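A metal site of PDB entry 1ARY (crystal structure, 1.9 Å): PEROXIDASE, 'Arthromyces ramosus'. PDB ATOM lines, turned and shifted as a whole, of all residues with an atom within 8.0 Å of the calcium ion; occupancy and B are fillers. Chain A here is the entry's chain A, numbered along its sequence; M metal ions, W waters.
Water W1 lies within hydrogen-bond range of the side-chain carboxylate (OE1) of Glu 87 and the backbone carbonyl oxygen (O) of His 56.
Four residues have an atom within 4 Å of the calcium ion: Asp 57, Gly 75, Asp 77 and Ser 79.
The calcium ion is bound by the side-chain carboxylate (OD1) of Asp 57 (2.4 Å).
The calcium ion is bound by OG of Ser 79.
The calcium ion is bound by the side-chain carboxylate (OD1) of Asp 77.
The calcium ion is bound by water W2 (2.4 Å).
The calcium ion is bound by O of Asp 57 (2.5 Å).
The calcium ion is bound by O of Gly 75 (2.5 Å).
Water W1 binds the calcium ion, 2.6 Å away.
The side-chain carboxylate (OD2) of Asp 57 is in hydrogen-bond range of the backbone NH (N) of Gly 78, 2.9 Å away.
The side-chain hydroxyl of Ser 79 lies close to the side-chain carboxylate of Glu 87 (2.6 Å).
The backbone NH (N) of Gly 75 sits at hydrogen-bond distance from the backbone carbonyl oxygen (O) of Gly 60 (3.1 Å).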
ATOM      1  N   ILE A  53     -19.286 -29.888   7.170  1.00  0.00           N
ATOM      2  CA  ILE A  53     -19.913 -28.608   6.841  1.00  0.00           C
ATOM      3  C   ILE A  53     -20.556 -28.552   5.437  1.00  0.00           C
ATOM      4  O   ILE A  53     -21.654 -27.989   5.303  1.00  0.00           O
ATOM      5  CB  ILE A  53     -18.830 -27.485   7.009  1.00  0.00           C
ATOM      6  CG1 ILE A  53     -18.514 -27.338   8.508  1.00  0.00           C
ATOM      7  CG2 ILE A  53     -19.315 -26.140   6.456  1.00  0.00           C
ATOM      8  CD1 ILE A  53     -17.299 -26.427   8.770  1.00  0.00           C
ATOM      9  N   VAL A  54     -19.925 -29.098   4.384  1.00  0.00           N
ATOM     10  CA  VAL A  54     -20.483 -29.042   3.031  1.00  0.00           C
ATOM     11  C   VAL A  54     -21.810 -29.827   3.005  1.00  0.00           C
ATOM     12  O   VAL A  54     -22.823 -29.309   2.535  1.00  0.00           O
ATOM     13  CB  VAL A  54     -19.368 -29.600   2.065  1.00  0.00           C
ATOM     14  CG1 VAL A  54     -19.188 -31.092   2.147  1.00  0.00           C
ATOM     15  CG2 VAL A  54     -19.745 -29.200   0.652  1.00  0.00           C
ATOM     16  N   PHE A  55     -21.848 -30.996   3.650  1.00  0.00           N
ATOM     17  CA  PHE A  55     -23.033 -31.816   3.770  1.00  0.00           C
ATOM     18  C   PHE A  55     -24.068 -31.068   4.582  1.00  0.00           C
ATOM     19  O   PHE A  55     -25.194 -30.904   4.098  1.00  0.00           O
ATOM     20  CB  PHE A  55     -22.711 -33.145   4.470  1.00  0.00           C
ATOM     21  CG  PHE A  55     -23.928 -34.070   4.685  1.00  0.00           C
ATOM     22  CD1 PHE A  55     -24.903 -34.229   3.715  1.00  0.00           C
ATOM     23  CD2 PHE A  55     -24.050 -34.747   5.874  1.00  0.00           C
ATOM     24  CE1 PHE A  55     -25.996 -35.049   3.951  1.00  0.00           C
ATOM     25  CE2 PHE A  55     -25.136 -35.568   6.103  1.00  0.00           C
ATOM     26  CZ  PHE A  55     -26.120 -35.713   5.151  1.00  0.00           C
ATOM     27  N   HIS A  56     -23.761 -30.580   5.780  1.00  0.00           N
ATOM     28  CA  HIS A  56     -24.757 -29.887   6.597  1.00  0.00           C
ATOM     29  C   HIS A  56     -25.243 -28.573   6.015  1.00  0.00           C
ATOM     30  O   HIS A  56     -26.384 -28.146   6.294  1.00  0.00           O
ATOM     31  CB  HIS A  56     -24.155 -29.720   7.990  1.00  0.00           C
ATOM     32  CG  HIS A  56     -24.227 -31.056   8.734  1.00  0.00           C
ATOM     33  ND1 HIS A  56     -23.966 -31.220  10.084  1.00  0.00           N
ATOM     34  CD2 HIS A  56     -24.575 -32.273   8.161  1.00  0.00           C
ATOM     35  CE1 HIS A  56     -24.138 -32.531  10.312  1.00  0.00           C
ATOM     36  NE2 HIS A  56     -24.484 -33.160   9.233  1.00  0.00           N
ATOM     37  N   ASP A  57     -24.439 -27.901   5.190  1.00  0.00           N
ATOM     38  CA  ASP A  57     -24.910 -26.703   4.533  1.00  0.00           C
ATOM     39  C   ASP A  57     -25.877 -27.124   3.434  1.00  0.00           C
ATOM     40  O   ASP A  57     -26.991 -26.558   3.386  1.00  0.00           O
ATOM     41  CB  ASP A  57     -23.781 -25.899   3.876  1.00  0.00           C
ATOM     42  CG  ASP A  57     -24.229 -24.629   3.162  1.00  0.00           C
ATOM     43  OD1 ASP A  57     -25.173 -23.993   3.622  1.00  0.00           O
ATOM     44  OD2 ASP A  57     -23.641 -24.254   2.159  1.00  0.00           O
ATOM     45  N   ALA A  58     -25.516 -28.118   2.606  1.00  0.00           N
ATOM     46  CA  ALA A  58     -26.330 -28.477   1.476  1.00  0.00           C
ATOM     47  C   ALA A  58     -27.628 -29.204   1.760  1.00  0.00           C
ATOM     48  O   ALA A  58     -28.660 -28.925   1.145  1.00  0.00           O
ATOM     49  CB  ALA A  58     -25.514 -29.316   0.536  1.00  0.00           C
ATOM     50  N   ILE A  59     -27.616 -30.085   2.759  1.00  0.00           N
ATOM     51  CA  ILE A  59     -28.801 -30.837   3.065  1.00  0.00           C
ATOM     52  C   ILE A  59     -29.944 -29.996   3.658  1.00  0.00           C
ATOM     53  O   ILE A  59     -31.063 -30.517   3.776  1.00  0.00           O
ATOM     54  CB  ILE A  59     -28.324 -32.049   3.986  1.00  0.00           C
ATOM     55  CG1 ILE A  59     -29.246 -33.253   3.733  1.00  0.00           C
ATOM     56  CG2 ILE A  59     -28.284 -31.651   5.467  1.00  0.00           C
ATOM     57  CD1 ILE A  59     -29.276 -33.702   2.253  1.00  0.00           C
ATOM     58  N   GLY A  60     -29.770 -28.721   4.003  1.00  0.00           N
ATOM     59  CA  GLY A  60     -30.850 -27.908   4.535  1.00  0.00           C
ATOM     60  C   GLY A  60     -31.600 -27.413   3.313  1.00  0.00           C
ATOM     61  O   GLY A  60     -31.535 -26.244   2.892  1.00  0.00           O
ATOM     62  N   PHE A  61     -32.316 -28.353   2.723  1.00  0.00           N
ATOM     63  CA  PHE A  61     -33.053 -28.121   1.499  1.00  0.00           C
ATOM     64  C   PHE A  61     -34.152 -29.166   1.527  1.00  0.00           C
ATOM     65  O   PHE A  61     -33.830 -30.345   1.645  1.00  0.00           O
ATOM     66  CB  PHE A  61     -32.108 -28.338   0.325  1.00  0.00           C
ATOM     67  CG  PHE A  61     -32.768 -28.196  -1.031  1.00  0.00           C
ATOM     68  CD1 PHE A  61     -33.082 -26.961  -1.489  1.00  0.00           C
ATOM     69  CD2 PHE A  61     -33.070 -29.345  -1.754  1.00  0.00           C
ATOM     70  CE1 PHE A  61     -33.717 -26.847  -2.709  1.00  0.00           C
ATOM     71  CE2 PHE A  61     -33.698 -29.228  -2.967  1.00  0.00           C
ATOM     72  CZ  PHE A  61     -34.031 -27.971  -3.448  1.00  0.00           C
ATOM     73  N   GLY A  73     -35.441 -24.025   2.787  1.00  0.00           N
ATOM     74  CA  GLY A  73     -33.989 -23.950   2.919  1.00  0.00           C
ATOM     75  C   GLY A  73     -33.432 -23.697   1.537  1.00  0.00           C
ATOM     76  O   GLY A  73     -34.080 -24.063   0.561  1.00  0.00           O
ATOM     77  N   GLY A  74     -32.289 -23.039   1.433  1.00  0.00           N
ATOM     78  CA  GLY A  74     -31.641 -22.742   0.177  1.00  0.00           C
ATOM     79  C   GLY A  74     -30.535 -23.704  -0.235  1.00  0.00           C
ATOM     80  O   GLY A  74     -29.780 -23.383  -1.167  1.00  0.00           O
ATOM     81  N   GLY A  75     -30.352 -24.863   0.413  1.00  0.00           N
ATOM     82  CA  GLY A  75     -29.357 -25.806  -0.004  1.00  0.00           C
ATOM     83  C   GLY A  75     -27.946 -25.327   0.221  1.00  0.00           C
ATOM     84  O   GLY A  75     -27.635 -24.820   1.303  1.00  0.00           O
ATOM     85  N   ALA A  76     -27.091 -25.454  -0.779  1.00  0.00           N
ATOM     86  CA  ALA A  76     -25.678 -25.091  -0.690  1.00  0.00           C
ATOM     87  C   ALA A  76     -25.486 -23.584  -0.811  1.00  0.00           C
ATOM     88  O   ALA A  76     -24.735 -23.095  -1.644  1.00  0.00           O
ATOM     89  CB  ALA A  76     -24.931 -25.826  -1.805  1.00  0.00           C
ATOM     90  N   ASP A  77     -26.084 -22.828   0.109  1.00  0.00           N
ATOM     91  CA  ASP A  77     -26.069 -21.374   0.095  1.00  0.00           C
ATOM     92  C   ASP A  77     -25.140 -20.669   1.108  1.00  0.00           C
ATOM     93  O   ASP A  77     -25.171 -19.444   1.277  1.00  0.00           O
ATOM     94  CB  ASP A  77     -27.522 -20.928   0.282  1.00  0.00           C
ATOM     95  CG  ASP A  77     -28.182 -21.428   1.575  1.00  0.00           C
ATOM     96  OD1 ASP A  77     -27.588 -22.184   2.354  1.00  0.00           O
ATOM     97  OD2 ASP A  77     -29.341 -21.060   1.812  1.00  0.00           O
ATOM     98  N   GLY A  78     -24.327 -21.433   1.830  1.00  0.00           N
ATOM     99  CA  GLY A  78     -23.453 -20.856   2.840  1.00  0.00           C
ATOM    100  C   GLY A  78     -24.207 -20.398   4.095  1.00  0.00           C
ATOM    101  O   GLY A  78     -23.624 -19.718   4.953  1.00  0.00           O
ATOM    102  N   SER A  79     -25.464 -20.840   4.276  1.00  0.00           N
ATOM    103  CA  SER A  79     -26.288 -20.425   5.400  1.00  0.00           C
ATOM    104  C   SER A  79     -25.692 -20.909   6.719  1.00  0.00           C
ATOM    105  O   SER A  79     -25.852 -20.231   7.742  1.00  0.00           O
ATOM    106  CB  SER A  79     -27.689 -20.960   5.192  1.00  0.00           C
ATOM    107  OG  SER A  79     -27.731 -22.386   5.351  1.00  0.00           O
ATOM    108  N   ILE A  80     -25.009 -22.056   6.755  1.00  0.00           N
ATOM    109  CA  ILE A  80     -24.363 -22.497   7.976  1.00  0.00           C
ATOM    110  C   ILE A  80     -23.343 -21.481   8.490  1.00  0.00           C
ATOM    111  O   ILE A  80     -23.075 -21.440   9.677  1.00  0.00           O
ATOM    112  CB  ILE A  80     -23.755 -23.913   7.702  1.00  0.00           C
ATOM    113  CG1 ILE A  80     -23.448 -24.620   9.023  1.00  0.00           C
ATOM    114  CG2 ILE A  80     -22.546 -23.786   6.798  1.00  0.00           C
ATOM    115  CD1 ILE A  80     -22.999 -26.083   8.863  1.00  0.00           C
ATOM    116  N   ILE A  81     -22.781 -20.600   7.632  1.00  0.00           N
ATOM    117  CA  ILE A  81     -21.836 -19.561   8.060  1.00  0.00           C
ATOM    118  C   ILE A  81     -22.604 -18.283   8.290  1.00  0.00           C
ATOM    119  O   ILE A  81     -22.583 -17.729   9.391  1.00  0.00           O
ATOM    120  CB  ILE A  81     -20.745 -19.302   6.999  1.00  0.00           C
ATOM    121  CG1 ILE A  81     -19.933 -20.582   6.801  1.00  0.00           C
ATOM    122  CG2 ILE A  81     -19.856 -18.120   7.440  1.00  0.00           C
ATOM    123  CD1 ILE A  81     -18.840 -20.558   5.736  1.00  0.00           C
ATOM    124  N   HIS A  83     -25.654 -17.710   8.881  1.00  0.00           N
ATOM    125  CA  HIS A  83     -26.579 -17.827   9.993  1.00  0.00           C
ATOM    126  C   HIS A  83     -26.065 -18.887  10.937  1.00  0.00           C
ATOM    127  O   HIS A  83     -26.826 -19.690  11.478  1.00  0.00           O
ATOM    128  CB  HIS A  83     -27.982 -18.223   9.515  1.00  0.00           C
ATOM    129  CG  HIS A  83     -28.512 -17.186   8.539  1.00  0.00           C
ATOM    130  ND1 HIS A  83     -28.918 -15.891   8.885  1.00  0.00           N
ATOM    131  CD2 HIS A  83     -28.506 -17.374   7.162  1.00  0.00           C
ATOM    132  CE1 HIS A  83     -29.104 -15.297   7.678  1.00  0.00           C
ATOM    133  NE2 HIS A  83     -28.875 -16.117   6.701  1.00  0.00           N
ATOM    134  N   GLU A  87     -27.851 -21.974  12.999  1.00  0.00           N
ATOM    135  CA  GLU A  87     -27.554 -23.342  12.617  1.00  0.00           C
ATOM    136  C   GLU A  87     -26.631 -24.160  13.480  1.00  0.00           C
ATOM    137  O   GLU A  87     -26.813 -25.379  13.598  1.00  0.00           O
ATOM    138  CB  GLU A  87     -27.022 -23.336  11.173  1.00  0.00           C
ATOM    139  CG  GLU A  87     -28.141 -22.886  10.235  1.00  0.00           C
ATOM    140  CD  GLU A  87     -27.908 -23.277   8.785  1.00  0.00           C
ATOM    141  OE1 GLU A  87     -27.307 -24.318   8.526  1.00  0.00           O
ATOM    142  OE2 GLU A  87     -28.340 -22.539   7.919  1.00  0.00           O
ATOM    143  N   GLY A 115     -21.310 -19.706   0.101  1.00  0.00           N
ATOM    144  CA  GLY A 115     -21.731 -20.956  -0.534  1.00  0.00           C
ATOM    145  C   GLY A 115     -20.654 -21.463  -1.488  1.00  0.00           C
ATOM    146  O   GLY A 115     -20.355 -22.669  -1.512  1.00  0.00           O
ATOM    147  N   ILE A 118     -17.518 -22.716   0.638  1.00  0.00           N
ATOM    148  CA  ILE A 118     -17.606 -24.043   1.215  1.00  0.00           C
ATOM    149  C   ILE A 118     -17.366 -25.103   0.140  1.00  0.00           C
ATOM    150  O   ILE A 118     -16.664 -26.100   0.450  1.00  0.00           O
ATOM    151  CB  ILE A 118     -18.985 -24.208   1.890  1.00  0.00           C
ATOM    152  CG1 ILE A 118     -19.102 -23.307   3.131  1.00  0.00           C
ATOM    153  CG2 ILE A 118     -19.112 -25.659   2.361  1.00  0.00           C
ATOM    154  CD1 ILE A 118     -20.495 -23.244   3.797  1.00  0.00           C
ATOM    155  N   SER A 145     -28.616 -15.670   2.014  1.00  0.00           N
ATOM    156  CA  SER A 145     -29.281 -16.862   2.477  1.00  0.00           C
ATOM    157  C   SER A 145     -30.174 -16.539   3.653  1.00  0.00           C
ATOM    158  O   SER A 145     -30.193 -15.438   4.206  1.00  0.00           O
ATOM    159  CB  SER A 145     -28.242 -17.897   2.909  1.00  0.00           C
ATOM    160  OG  SER A 145     -27.371 -17.376   3.906  1.00  0.00           O
ATOM    161  N   GLN A 146     -31.065 -17.478   3.900  1.00  0.00           N
ATOM    162  CA  GLN A 146     -31.949 -17.430   5.039  1.00  0.00           C
ATOM    163  C   GLN A 146     -31.500 -18.637   5.853  1.00  0.00           C
ATOM    164  O   GLN A 146     -30.882 -19.558   5.286  1.00  0.00           O
ATOM    165  CB  GLN A 146     -33.385 -17.615   4.608  1.00  0.00           C
ATOM    166  CG  GLN A 146     -34.035 -16.349   4.074  1.00  0.00           C
ATOM    167  CD  GLN A 146     -35.254 -16.712   3.245  1.00  0.00           C
ATOM    168  OE1 GLN A 146     -36.343 -17.030   3.732  1.00  0.00           O
ATOM    169  NE2 GLN A 146     -35.070 -16.701   1.924  1.00  0.00           N
ATOM    170  N   PRO A 147     -31.747 -18.700   7.185  1.00  0.00           N
ATOM    171  CA  PRO A 147     -31.439 -19.843   8.015  1.00  0.00           C
ATOM    172  C   PRO A 147     -32.181 -21.073   7.501  1.00  0.00           C
ATOM    173  O   PRO A 147     -33.328 -20.995   7.063  1.00  0.00           O
ATOM    174  CB  PRO A 147     -31.888 -19.482   9.393  1.00  0.00           C
ATOM    175  CG  PRO A 147     -31.946 -17.987   9.384  1.00  0.00           C
ATOM    176  CD  PRO A 147     -32.398 -17.650   7.985  1.00  0.00           C
ATOM    177  N   SER A 148     -31.469 -22.185   7.565  1.00  0.00           N
ATOM    178  CA  SER A 148     -32.007 -23.474   7.222  1.00  0.00           C
ATOM    179  C   SER A 148     -33.047 -23.817   8.289  1.00  0.00           C
ATOM    180  O   SER A 148     -32.885 -23.444   9.475  1.00  0.00           O
ATOM    181  CB  SER A 148     -30.911 -24.519   7.240  1.00  0.00           C
ATOM    182  OG  SER A 148     -31.353 -25.879   7.265  1.00  0.00           O
ATOM    183  N   PRO A 149     -34.168 -24.455   7.924  1.00  0.00           N
ATOM    184  CA  PRO A 149     -35.112 -24.960   8.889  1.00  0.00           C
ATOM    185  C   PRO A 149     -34.419 -26.015   9.777  1.00  0.00           C
ATOM    186  O   PRO A 149     -33.404 -26.605   9.390  1.00  0.00           O
ATOM    187  CB  PRO A 149     -36.239 -25.501   8.015  1.00  0.00           C
ATOM    188  CG  PRO A 149     -36.184 -24.653   6.764  1.00  0.00           C
ATOM    189  CD  PRO A 149     -34.688 -24.526   6.551  1.00  0.00           C
ATOM    190  N   LEU A 283     -27.622 -28.108  -4.885  1.00  0.00           N
ATOM    191  CA  LEU A 283     -28.945 -28.222  -4.288  1.00  0.00           C
ATOM    192  C   LEU A 283     -29.337 -26.770  -3.958  1.00  0.00           C
ATOM    193  O   LEU A 283     -28.590 -26.031  -3.315  1.00  0.00           O
ATOM    194  CB  LEU A 283     -28.816 -29.091  -3.041  1.00  0.00           C
ATOM    195  CG  LEU A 283     -29.545 -30.426  -2.903  1.00  0.00           C
ATOM    196  CD1 LEU A 283     -29.310 -31.341  -4.087  1.00  0.00           C
ATOM    197  CD2 LEU A 283     -29.113 -31.032  -1.573  1.00  0.00           C
ATOM    198  N   PHE A 285     -29.758 -24.509  -6.477  1.00  0.00           N
ATOM    199  CA  PHE A 285     -29.295 -23.695  -7.602  1.00  0.00           C
ATOM    200  C   PHE A 285     -29.464 -24.408  -8.924  1.00  0.00           C
ATOM    201  O   PHE A 285     -29.757 -25.603  -9.005  1.00  0.00           O
ATOM    202  CB  PHE A 285     -27.777 -23.321  -7.472  1.00  0.00           C
ATOM    203  CG  PHE A 285     -27.505 -22.502  -6.211  1.00  0.00           C
ATOM    204  CD1 PHE A 285     -27.310 -23.147  -5.004  1.00  0.00           C
ATOM    205  CD2 PHE A 285     -27.554 -21.133  -6.256  1.00  0.00           C
ATOM    206  CE1 PHE A 285     -27.166 -22.404  -3.847  1.00  0.00           C
ATOM    207  CE2 PHE A 285     -27.415 -20.403  -5.102  1.00  0.00           C
ATOM    208  CZ  PHE A 285     -27.221 -21.039  -3.898  1.00  0.00           C
HETATM  209 CA    CA M   1     -27.529 -24.179   3.743  1.00  0.00          CA
HETATM  210  O   HOH W   1     -27.754 -25.471   5.970  1.00  0.00           O
HETATM  211  O   HOH W   2     -29.959 -24.426   3.922  1.00  0.00           O
